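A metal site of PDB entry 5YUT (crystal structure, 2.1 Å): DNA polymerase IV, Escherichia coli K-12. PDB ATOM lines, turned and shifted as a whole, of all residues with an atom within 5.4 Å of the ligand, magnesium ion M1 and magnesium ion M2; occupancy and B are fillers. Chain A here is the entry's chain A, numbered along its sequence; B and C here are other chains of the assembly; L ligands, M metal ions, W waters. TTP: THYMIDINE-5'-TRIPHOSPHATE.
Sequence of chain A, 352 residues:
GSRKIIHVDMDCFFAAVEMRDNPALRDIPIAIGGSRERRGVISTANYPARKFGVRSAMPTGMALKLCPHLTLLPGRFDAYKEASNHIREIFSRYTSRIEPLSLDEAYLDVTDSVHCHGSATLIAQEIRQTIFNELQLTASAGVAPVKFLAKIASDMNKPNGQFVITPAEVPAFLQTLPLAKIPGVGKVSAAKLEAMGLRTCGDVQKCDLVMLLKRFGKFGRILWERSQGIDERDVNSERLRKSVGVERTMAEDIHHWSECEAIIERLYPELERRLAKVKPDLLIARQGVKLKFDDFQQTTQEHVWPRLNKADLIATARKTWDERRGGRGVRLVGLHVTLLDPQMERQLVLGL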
ATOM      1  N   ASP A   9      18.605 -12.677  17.932  1.00  0.00           N
ATOM      2  CA  ASP A   9      19.185 -12.649  19.280  1.00  0.00           C
ATOM      3  C   ASP A   9      18.067 -12.882  20.302  1.00  0.00           C
ATOM      4  O   ASP A   9      17.083 -12.139  20.311  1.00  0.00           O
ATOM      5  CB  ASP A   9      19.875 -11.286  19.527  1.00  0.00           C
ATOM      6  CG  ASP A   9      20.708 -11.242  20.817  1.00  0.00           C
ATOM      7  OD1 ASP A   9      20.144 -11.305  21.933  1.00  0.00           O
ATOM      8  OD2 ASP A   9      21.948 -11.063  20.718  1.00  0.00           O
ATOM      9  N   MET A  10      18.225 -13.891  21.159  1.00  0.00           N
ATOM     10  CA  MET A  10      17.211 -14.155  22.181  1.00  0.00           C
ATOM     11  C   MET A  10      17.235 -13.071  23.254  1.00  0.00           C
ATOM     12  O   MET A  10      18.268 -12.476  23.544  1.00  0.00           O
ATOM     13  CB  MET A  10      17.446 -15.514  22.849  1.00  0.00           C
ATOM     14  CG  MET A  10      17.574 -16.708  21.911  1.00  0.00           C
ATOM     15  SD  MET A  10      15.999 -17.103  21.138  1.00  0.00           S
ATOM     16  CE  MET A  10      14.980 -17.405  22.584  1.00  0.00           C
ATOM     17  N   ASP A  11      16.077 -12.833  23.863  1.00  0.00           N
ATOM     18  CA  ASP A  11      15.929 -11.802  24.883  1.00  0.00           C
ATOM     19  C   ASP A  11      16.229 -12.374  26.268  1.00  0.00           C
ATOM     20  O   ASP A  11      15.620 -13.369  26.682  1.00  0.00           O
ATOM     21  CB  ASP A  11      14.507 -11.226  24.855  1.00  0.00           C
ATOM     22  CG  ASP A  11      14.154 -10.591  23.515  1.00  0.00           C
ATOM     23  OD1 ASP A  11      14.900  -9.697  23.076  1.00  0.00           O
ATOM     24  OD2 ASP A  11      13.112 -10.979  22.918  1.00  0.00           O
ATOM     25  N   CYS A  12      17.150 -11.714  26.989  1.00  0.00           N
ATOM     26  CA  CYS A  12      17.562 -12.083  28.351  1.00  0.00           C
ATOM     27  C   CYS A  12      17.641 -13.591  28.539  1.00  0.00           C
ATOM     28  O   CYS A  12      17.001 -14.187  29.402  1.00  0.00           O
ATOM     29  CB  CYS A  12      16.630 -11.456  29.386  1.00  0.00           C
ATOM     30  SG  CYS A  12      16.486  -9.679  29.250  1.00  0.00           S
ATOM     31  N   PHE A  13      18.483 -14.198  27.694  1.00  0.00           N
ATOM     32  CA  PHE A  13      18.364 -15.610  27.376  1.00  0.00           C
ATOM     33  C   PHE A  13      18.314 -16.494  28.620  1.00  0.00           C
ATOM     34  O   PHE A  13      17.359 -17.246  28.814  1.00  0.00           O
ATOM     35  CB  PHE A  13      19.499 -16.033  26.445  1.00  0.00           C
ATOM     36  CG  PHE A  13      19.448 -17.480  26.046  1.00  0.00           C
ATOM     37  CD1 PHE A  13      18.259 -18.049  25.603  1.00  0.00           C
ATOM     38  CD2 PHE A  13      20.591 -18.258  26.081  1.00  0.00           C
ATOM     39  CE1 PHE A  13      18.203 -19.383  25.224  1.00  0.00           C
ATOM     40  CE2 PHE A  13      20.559 -19.591  25.706  1.00  0.00           C
ATOM     41  CZ  PHE A  13      19.357 -20.154  25.264  1.00  0.00           C
ATOM     42  N   PHE A  14      19.345 -16.424  29.469  1.00  0.00           N
ATOM     43  CA  PHE A  14      19.354 -17.315  30.634  1.00  0.00           C
ATOM     44  C   PHE A  14      18.157 -17.056  31.528  1.00  0.00           C
ATOM     45  O   PHE A  14      17.538 -17.998  32.027  1.00  0.00           O
ATOM     46  CB  PHE A  14      20.648 -17.170  31.447  1.00  0.00           C
ATOM     47  CG  PHE A  14      21.867 -17.778  30.794  1.00  0.00           C
ATOM     48  CD1 PHE A  14      21.829 -18.237  29.484  1.00  0.00           C
ATOM     49  CD2 PHE A  14      23.061 -17.866  31.504  1.00  0.00           C
ATOM     50  CE1 PHE A  14      22.950 -18.776  28.893  1.00  0.00           C
ATOM     51  CE2 PHE A  14      24.172 -18.409  30.923  1.00  0.00           C
ATOM     52  CZ  PHE A  14      24.129 -18.864  29.620  1.00  0.00           C
ATOM     53  N   ALA A  15      17.813 -15.780  31.754  1.00  0.00           N
ATOM     54  CA  ALA A  15      16.698 -15.437  32.642  1.00  0.00           C
ATOM     55  C   ALA A  15      15.343 -15.783  32.033  1.00  0.00           C
ATOM     56  O   ALA A  15      14.404 -16.109  32.767  1.00  0.00           O
ATOM     57  CB  ALA A  15      16.743 -13.954  32.997  1.00  0.00           C
ATOM     58  N   ILE A  42      27.493 -11.313  37.526  1.00  0.00           N
ATOM     59  CA  ILE A  42      26.167 -11.528  36.936  1.00  0.00           C
ATOM     60  C   ILE A  42      26.347 -11.978  35.486  1.00  0.00           C
ATOM     61  O   ILE A  42      27.030 -11.301  34.701  1.00  0.00           O
ATOM     62  CB  ILE A  42      25.310 -10.252  37.009  1.00  0.00           C
ATOM     63  CG1 ILE A  42      25.081  -9.835  38.458  1.00  0.00           C
ATOM     64  CG2 ILE A  42      23.974 -10.451  36.256  1.00  0.00           C
ATOM     65  CD1 ILE A  42      24.477 -10.914  39.320  1.00  0.00           C
ATOM     66  N   SER A  43      25.728 -13.110  35.121  1.00  0.00           N
ATOM     67  CA  SER A  43      25.716 -13.562  33.725  1.00  0.00           C
ATOM     68  C   SER A  43      24.683 -12.811  32.901  1.00  0.00           C
ATOM     69  O   SER A  43      24.973 -12.310  31.805  1.00  0.00           O
ATOM     70  CB  SER A  43      25.464 -15.069  33.643  1.00  0.00           C
ATOM     71  OG  SER A  43      26.666 -15.823  33.666  1.00  0.00           O
ATOM     72  N   THR A  44      23.451 -12.741  33.396  1.00  0.00           N
ATOM     73  CA  THR A  44      22.446 -11.867  32.811  1.00  0.00           C
ATOM     74  C   THR A  44      21.353 -11.655  33.848  1.00  0.00           C
ATOM     75  O   THR A  44      21.336 -12.286  34.901  1.00  0.00           O
ATOM     76  CB  THR A  44      21.882 -12.448  31.508  1.00  0.00           C
ATOM     77  OG1 THR A  44      21.130 -11.438  30.838  1.00  0.00           O
ATOM     78  CG2 THR A  44      20.985 -13.628  31.810  1.00  0.00           C
ATOM     79  N   ALA A  45      20.417 -10.779  33.516  1.00  0.00           N
ATOM     80  CA  ALA A  45      19.321 -10.445  34.410  1.00  0.00           C
ATOM     81  C   ALA A  45      18.065 -10.182  33.590  1.00  0.00           C
ATOM     82  O   ALA A  45      18.127  -9.859  32.395  1.00  0.00           O
ATOM     83  CB  ALA A  45      19.661  -9.224  35.274  1.00  0.00           C
ATOM     84  N   TYR A  47      14.356  -8.040  33.036  1.00  0.00           N
ATOM     85  CA  TYR A  47      14.085  -6.601  32.990  1.00  0.00           C
ATOM     86  C   TYR A  47      13.755  -6.006  34.355  1.00  0.00           C
ATOM     87  O   TYR A  47      14.152  -4.854  34.591  1.00  0.00           O
ATOM     88  CB  TYR A  47      12.986  -6.320  31.948  1.00  0.00           C
ATOM     89  CG  TYR A  47      13.566  -6.249  30.566  1.00  0.00           C
ATOM     90  CD1 TYR A  47      14.228  -5.104  30.119  1.00  0.00           C
ATOM     91  CD2 TYR A  47      13.513  -7.349  29.711  1.00  0.00           C
ATOM     92  CE1 TYR A  47      14.793  -5.051  28.852  1.00  0.00           C
ATOM     93  CE2 TYR A  47      14.074  -7.304  28.446  1.00  0.00           C
ATOM     94  CZ  TYR A  47      14.715  -6.153  28.023  1.00  0.00           C
ATOM     95  OH  TYR A  47      15.265  -6.099  26.772  1.00  0.00           O
ATOM     96  N   ARG A  50      17.019  -5.235  35.716  1.00  0.00           N
ATOM     97  CA  ARG A  50      17.745  -4.246  34.924  1.00  0.00           C
ATOM     98  C   ARG A  50      17.349  -2.811  35.245  1.00  0.00           C
ATOM     99  O   ARG A  50      18.180  -1.902  35.091  1.00  0.00           O
ATOM    100  CB  ARG A  50      17.527  -4.524  33.437  1.00  0.00           C
ATOM    101  CG  ARG A  50      18.187  -5.800  33.010  1.00  0.00           C
ATOM    102  CD  ARG A  50      18.182  -6.052  31.511  1.00  0.00           C
ATOM    103  NE  ARG A  50      18.853  -7.329  31.265  1.00  0.00           N
ATOM    104  CZ  ARG A  50      19.274  -7.723  30.078  1.00  0.00           C
ATOM    105  NH1 ARG A  50      19.083  -6.983  28.992  1.00  0.00           N
ATOM    106  NH2 ARG A  50      19.874  -8.924  29.970  1.00  0.00           N
ATOM    107  N   SER A  56      24.854  -7.614  32.821  1.00  0.00           N
ATOM    108  CA  SER A  56      25.841  -8.652  32.599  1.00  0.00           C
ATOM    109  C   SER A  56      27.222  -8.141  32.985  1.00  0.00           C
ATOM    110  O   SER A  56      27.537  -6.967  32.826  1.00  0.00           O
ATOM    111  CB  SER A  56      25.815  -9.069  31.139  1.00  0.00           C
ATOM    112  OG  SER A  56      24.710  -9.912  30.905  1.00  0.00           O
ATOM    113  N   ALA A  57      28.042  -9.049  33.522  1.00  0.00           N
ATOM    114  CA  ALA A  57      29.432  -8.811  33.901  1.00  0.00           C
ATOM    115  C   ALA A  57      29.556  -7.956  35.165  1.00  0.00           C
ATOM    116  O   ALA A  57      30.673  -7.630  35.561  1.00  0.00           O
ATOM    117  CB  ALA A  57      30.254  -8.178  32.766  1.00  0.00           C
ATOM    118  N   SER A 102      26.939 -17.545  19.457  1.00  0.00           N
ATOM    119  CA  SER A 102      26.837 -17.953  20.851  1.00  0.00           C
ATOM    120  C   SER A 102      25.653 -18.908  20.893  1.00  0.00           C
ATOM    121  O   SER A 102      25.037 -19.201  19.856  1.00  0.00           O
ATOM    122  CB  SER A 102      26.638 -16.757  21.790  1.00  0.00           C
ATOM    123  OG  SER A 102      25.329 -16.205  21.679  1.00  0.00           O
ATOM    124  N   ASP A 104      22.793 -18.169  21.885  1.00  0.00           N
ATOM    125  CA  ASP A 104      21.519 -17.473  21.775  1.00  0.00           C
ATOM    126  C   ASP A 104      21.399 -16.563  20.556  1.00  0.00           C
ATOM    127  O   ASP A 104      20.392 -15.845  20.435  1.00  0.00           O
ATOM    128  CB  ASP A 104      21.247 -16.690  23.084  1.00  0.00           C
ATOM    129  CG  ASP A 104      21.624 -15.215  22.997  1.00  0.00           C
ATOM    130  OD1 ASP A 104      22.695 -14.871  22.439  1.00  0.00           O
ATOM    131  OD2 ASP A 104      20.832 -14.393  23.504  1.00  0.00           O
ATOM    132  N   GLU A 105      22.376 -16.559  19.654  1.00  0.00           N
ATOM    133  CA  GLU A 105      22.275 -15.690  18.492  1.00  0.00           C
ATOM    134  C   GLU A 105      22.981 -16.303  17.301  1.00  0.00           C
ATOM    135  O   GLU A 105      23.871 -17.141  17.441  1.00  0.00           O
ATOM    136  CB  GLU A 105      22.840 -14.281  18.796  1.00  0.00           C
ATOM    137  CG  GLU A 105      24.311 -14.238  19.127  1.00  0.00           C
ATOM    138  CD  GLU A 105      24.772 -12.832  19.555  1.00  0.00           C
ATOM    139  OE1 GLU A 105      25.293 -12.081  18.695  1.00  0.00           O
ATOM    140  OE2 GLU A 105      24.596 -12.472  20.739  1.00  0.00           O
ATOM    141  N   ASP A 155      19.130  -4.977  18.149  1.00  0.00           N
ATOM    142  CA  ASP A 155      19.004  -4.435  19.492  1.00  0.00           C
ATOM    143  C   ASP A 155      18.085  -3.217  19.571  1.00  0.00           C
ATOM    144  O   ASP A 155      17.796  -2.750  20.682  1.00  0.00           O
ATOM    145  CB  ASP A 155      20.385  -4.113  20.066  1.00  0.00           C
ATOM    146  CG  ASP A 155      20.913  -5.225  20.948  1.00  0.00           C
ATOM    147  OD1 ASP A 155      20.817  -6.405  20.547  1.00  0.00           O
ATOM    148  OD2 ASP A 155      21.393  -4.935  22.055  1.00  0.00           O
ATOM    149  N   LYS A 158      14.487  -4.438  20.863  1.00  0.00           N
ATOM    150  CA  LYS A 158      14.424  -5.479  21.901  1.00  0.00           C
ATOM    151  C   LYS A 158      13.645  -4.945  23.090  1.00  0.00           C
ATOM    152  O   LYS A 158      13.744  -3.770  23.396  1.00  0.00           O
ATOM    153  CB  LYS A 158      15.814  -5.902  22.403  1.00  0.00           C
ATOM    154  CG  LYS A 158      16.683  -6.655  21.462  1.00  0.00           C
ATOM    155  CD  LYS A 158      17.998  -7.060  22.138  1.00  0.00           C
ATOM    156  CE  LYS A 158      17.842  -8.348  22.915  1.00  0.00           C
ATOM    157  NZ  LYS A 158      18.004  -9.601  22.117  1.00  0.00           N
ATOM    158  P    DA B   4      35.813 -12.162  37.852  1.00  0.00           P
ATOM    159  OP1  DA B   4      36.877 -12.658  38.770  1.00  0.00           O
ATOM    160  OP2  DA B   4      36.177 -11.500  36.601  1.00  0.00           O
ATOM    161  O5'  DA B   4      34.799 -13.363  37.546  1.00  0.00           O
ATOM    162  C5'  DA B   4      34.151 -14.058  38.615  1.00  0.00           C
ATOM    163  C4'  DA B   4      33.650 -15.418  38.153  1.00  0.00           C
ATOM    164  O4'  DA B   4      32.628 -15.264  37.129  1.00  0.00           O
ATOM    165  C3'  DA B   4      34.707 -16.307  37.524  1.00  0.00           C
ATOM    166  O3'  DA B   4      34.370 -17.664  37.733  1.00  0.00           O
ATOM    167  C2'  DA B   4      34.644 -15.922  36.032  1.00  0.00           C
ATOM    168  C1'  DA B   4      33.147 -15.620  35.848  1.00  0.00           C
ATOM    169  N9   DA B   4      32.868 -14.521  34.921  1.00  0.00           N
ATOM    170  C8   DA B   4      33.590 -13.375  34.752  1.00  0.00           C
ATOM    171  N7   DA B   4      33.089 -12.549  33.855  1.00  0.00           N
ATOM    172  C5   DA B   4      31.951 -13.203  33.410  1.00  0.00           C
ATOM    173  C6   DA B   4      30.964 -12.848  32.461  1.00  0.00           C
ATOM    174  N6   DA B   4      30.986 -11.714  31.758  1.00  0.00           N
ATOM    175  N1   DA B   4      29.951 -13.715  32.272  1.00  0.00           N
ATOM    176  C2   DA B   4      29.935 -14.854  32.969  1.00  0.00           C
ATOM    177  N3   DA B   4      30.804 -15.296  33.886  1.00  0.00           N
ATOM    178  C4   DA B   4      31.800 -14.416  34.053  1.00  0.00           C
ATOM    179  P    DG B   5      35.372 -18.849  37.307  1.00  0.00           P
ATOM    180  OP1  DG B   5      35.220 -19.922  38.314  1.00  0.00           O
ATOM    181  OP2  DG B   5      36.727 -18.261  37.060  1.00  0.00           O
ATOM    182  O5'  DG B   5      34.879 -19.290  35.848  1.00  0.00           O
ATOM    183  C5'  DG B   5      33.598 -19.813  35.648  1.00  0.00           C
ATOM    184  C4'  DG B   5      33.386 -20.020  34.174  1.00  0.00           C
ATOM    185  O4'  DG B   5      33.103 -18.740  33.552  1.00  0.00           O
ATOM    186  C3'  DG B   5      34.621 -20.581  33.428  1.00  0.00           C
ATOM    187  O3'  DG B   5      34.218 -21.552  32.474  1.00  0.00           O
ATOM    188  C2'  DG B   5      35.198 -19.346  32.740  1.00  0.00           C
ATOM    189  C1'  DG B   5      33.917 -18.609  32.395  1.00  0.00           C
ATOM    190  N9   DG B   5      34.093 -17.205  32.058  1.00  0.00           N
ATOM    191  C8   DG B   5      35.038 -16.327  32.530  1.00  0.00           C
ATOM    192  N7   DG B   5      34.910 -15.118  32.020  1.00  0.00           N
ATOM    193  C5   DG B   5      33.813 -15.207  31.190  1.00  0.00           C
ATOM    194  C6   DG B   5      33.192 -14.230  30.357  1.00  0.00           C
ATOM    195  O6   DG B   5      33.500 -13.038  30.209  1.00  0.00           O
ATOM    196  N1   DG B   5      32.111 -14.752  29.664  1.00  0.00           N
ATOM    197  C2   DG B   5      31.682 -16.051  29.748  1.00  0.00           C
ATOM    198  N2   DG B   5      30.626 -16.385  28.989  1.00  0.00           N
ATOM    199  N3   DG B   5      32.249 -16.976  30.504  1.00  0.00           N
ATOM    200  C4   DG B   5      33.304 -16.489  31.187  1.00  0.00           C
ATOM    201  P    DC C  18      27.867  -9.541  21.503  1.00  0.00           P
ATOM    202  OP1  DC C  18      27.033  -9.619  20.294  1.00  0.00           O
ATOM    203  OP2  DC C  18      27.691  -8.410  22.461  1.00  0.00           O
ATOM    204  O5'  DC C  18      27.679 -10.876  22.345  1.00  0.00           O
ATOM    205  C5'  DC C  18      28.069 -12.116  21.799  1.00  0.00           C
ATOM    206  C4'  DC C  18      27.784 -13.214  22.806  1.00  0.00           C
ATOM    207  O4'  DC C  18      28.881 -13.310  23.720  1.00  0.00           O
ATOM    208  C3'  DC C  18      26.526 -12.976  23.641  1.00  0.00           C
ATOM    209  O3'  DC C  18      25.577 -13.993  23.403  1.00  0.00           O
ATOM    210  C2'  DC C  18      27.015 -12.971  25.108  1.00  0.00           C
ATOM    211  C1'  DC C  18      28.417 -13.569  25.020  1.00  0.00           C
ATOM    212  N1   DC C  18      29.346 -12.934  25.993  1.00  0.00           N
ATOM    213  C2   DC C  18      29.905 -13.699  27.007  1.00  0.00           C
ATOM    214  O2   DC C  18      29.642 -14.908  27.057  1.00  0.00           O
ATOM    215  N3   DC C  18      30.741 -13.087  27.895  1.00  0.00           N
ATOM    216  C4   DC C  18      31.006 -11.779  27.793  1.00  0.00           C
ATOM    217  N4   DC C  18      31.826 -11.215  28.686  1.00  0.00           N
ATOM    218  C5   DC C  18      30.424 -10.982  26.768  1.00  0.00           C
ATOM    219  C6   DC C  18      29.604 -11.594  25.907  1.00  0.00           C
HETATM  220  PA  TTP L   1      23.393 -11.683  25.423  1.00  0.00           P
HETATM  221  O1A TTP L   1      22.621 -11.932  24.133  1.00  0.00           O
HETATM  222  O2A TTP L   1      24.545 -10.751  25.157  1.00  0.00           O
HETATM  223  O3A TTP L   1      22.466 -11.036  26.577  1.00  0.00           O
HETATM  224  PB  TTP L   1      20.970 -11.500  26.962  1.00  0.00           P
HETATM  225  O1B TTP L   1      20.894 -12.072  28.359  1.00  0.00           O
HETATM  226  O2B TTP L   1      20.358 -12.521  26.024  1.00  0.00           O
HETATM  227  O3B TTP L   1      20.238 -10.074  26.971  1.00  0.00           O
HETATM  228  PG  TTP L   1      19.646  -9.348  25.642  1.00  0.00           P
HETATM  229  O1G TTP L   1      20.173 -10.010  24.361  1.00  0.00           O
HETATM  230  O2G TTP L   1      20.044  -7.882  25.678  1.00  0.00           O
HETATM  231  O3G TTP L   1      18.142  -9.465  25.681  1.00  0.00           O
HETATM  232  O5' TTP L   1      23.958 -13.023  26.102  1.00  0.00           O
HETATM  233  C5' TTP L   1      23.374 -14.321  25.908  1.00  0.00           C
HETATM  234  C4' TTP L   1      23.620 -15.099  27.206  1.00  0.00           C
HETATM  235  O4' TTP L   1      25.039 -15.184  27.441  1.00  0.00           O
HETATM  236  C3' TTP L   1      23.073 -14.412  28.455  1.00  0.00           C
HETATM  237  O3' TTP L   1      21.696 -14.720  28.710  1.00  0.00           O
HETATM  238  C2' TTP L   1      24.011 -14.896  29.555  1.00  0.00           C
HETATM  239  C1' TTP L   1      25.334 -15.182  28.832  1.00  0.00           C
HETATM  240  N1  TTP L   1      26.238 -14.068  29.083  1.00  0.00           N
HETATM  241  C2  TTP L   1      27.232 -14.195  30.069  1.00  0.00           C
HETATM  242  O2  TTP L   1      27.345 -15.284  30.686  1.00  0.00           O
HETATM  243  N3  TTP L   1      28.056 -13.190  30.362  1.00  0.00           N
HETATM  244  C4  TTP L   1      27.960 -12.023  29.718  1.00  0.00           C
HETATM  245  O4  TTP L   1      28.753 -11.108  30.005  1.00  0.00           O
HETATM  246  C5  TTP L   1      26.922 -11.840  28.689  1.00  0.00           C
HETATM  247  C5M TTP L   1      26.775 -10.538  27.942  1.00  0.00           C
HETATM  248  C6  TTP L   1      26.080 -12.912  28.413  1.00  0.00           C
HETATM  249 MG    MG M   1      23.169 -12.515  22.154  1.00  0.00          MG
HETATM  250 MG    MG M   2      20.586 -12.092  23.836  1.00  0.00          MG
HETATM  251  O   HOH W   1      27.963 -18.142  30.866  1.00  0.00           O
HETATM  252  O   HOH W   2      22.241  -8.921  22.970  1.00  0.00           O
HETATM  253  O   HOH W   3      24.628  -9.983  21.862  1.00  0.00           O
HETATM  254  O   HOH W   4      29.401  -8.462  29.181  1.00  0.00           O
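Lys 158 touches magnesium ion M2.
Four residues have an atom within 4 Å of magnesium ion M2: Asp 9, Met 10, Asp 104 and Lys 158.
Water W3 lies within hydrogen-bond range of OP1 of DC 18 of chain C (2.9 Å) and O2A of the ligand (3.4 Å).
OG1 of Thr 44 lies within hydrogen-bond range of O1B of the ligand, at 2.6 Å.
N1 of DA 4 of chain B is in hydrogen-bond range of N3 of the ligand, 2.7 Å away.
O3G of the ligand sits at hydrogen-bond distance from N of Cys 12 (2.8 Å).
NZ of Lys 158 is in salt-bridge range of O3G of the ligand (3.6 Å).
The backbone NH (N) of Phe 14 sits at hydrogen-bond distance from an oxygen (O3') of the ligand.
The backbone NH (N) of Phe 13 lies within hydrogen-bond range of an oxygen (O1B) of the ligand, at 3.3 Å.
An oxygen (O2) of the ligand is in hydrogen-bond range of the side-chain hydroxyl (OG) of Ser 43 (3.1 Å).
NH1 of Arg 50 is in salt-bridge range of O2G of the ligand, at 3.6 Å.
Magnesium ion M2 is bound by an oxygen (O1A) of the ligand (2.1 Å), the side-chain carboxylate of Asp 9 (2.1 Å), an oxygen (O1G) of the ligand (2.2 Å), an oxygen (O2B) of the ligand (2.2 Å), the side-chain carboxylate of Asp 104 (2.3 Å) and the backbone carbonyl oxygen of Met 10 (2.4 Å).
Magnesium ion M2 has six donor atoms within binding distance.
The backbone NH (N) of Asp 104 lies close to the side-chain hydroxyl (OG) of Ser 102 (3.2 Å).
The guanidinium group (NH2) of Arg 50 lies within hydrogen-bond range of the side-chain hydroxyl (OG1) of Thr 44 (2.9 Å).
The side-chain sulfur (SG) of Cys 12 sits close to the guanidinium group (NH2) of Arg 50, 3.5 Å away.
The backbone carbonyl oxygen (O) of Ala 45 sits at hydrogen-bond distance from the side-chain sulfur (SG) of Cys 12 (3.6 Å).
O2 of DC 18 of chain C sits close to N2 of DG 5 of chain B.
O3' of DC 18 of chain C sits at hydrogen-bond distance from OG of Ser 102 (2.8 Å).
The backbone carbonyl oxygen of Ser 43 lies within hydrogen-bond range of the side-chain hydroxyl of Ser 56.
The backbone carbonyl oxygen (O) of Ala 45 sits at hydrogen-bond distance from the guanidinium group (NE) of Arg 50, at 2.9 Å.
An oxygen (O5') of the ligand sits close to O3' of DC 18 of chain C (3.3 Å).
CA of Asp 11 touches O3G of the ligand (3.3 Å).
CB of Ser 56 touches C5M of the ligand (3.6 Å).
DG 5 of chain B touches the ligand (N2 to O2, 3.9 Å).
Hydrophobic or aromatic side chains that line the ligand: Phe 13 and Phe 14.
Along chain A the residues within 4 Å of the ligand span positions 9 to 158.
The nearest printed residue that does not touch the ligand is Ala 57 (4.1 Å).
Merely in contact with magnesium ion M1: DC 18 of chain C.
Four residues have an atom within 4 Å of magnesium ion M1: Asp 9, Asp 104, Glu 105 and DC 18 of chain C.
Magnesium ion M1 is bound by OE2 of Glu 105 (2.0 Å), O1A of the ligand (2.1 Å), OD2 of Asp 9 (2.4 Å) and OD1 of Asp 104 (2.4 Å).
Magnesium ion M1 has four donor atoms within binding distance.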
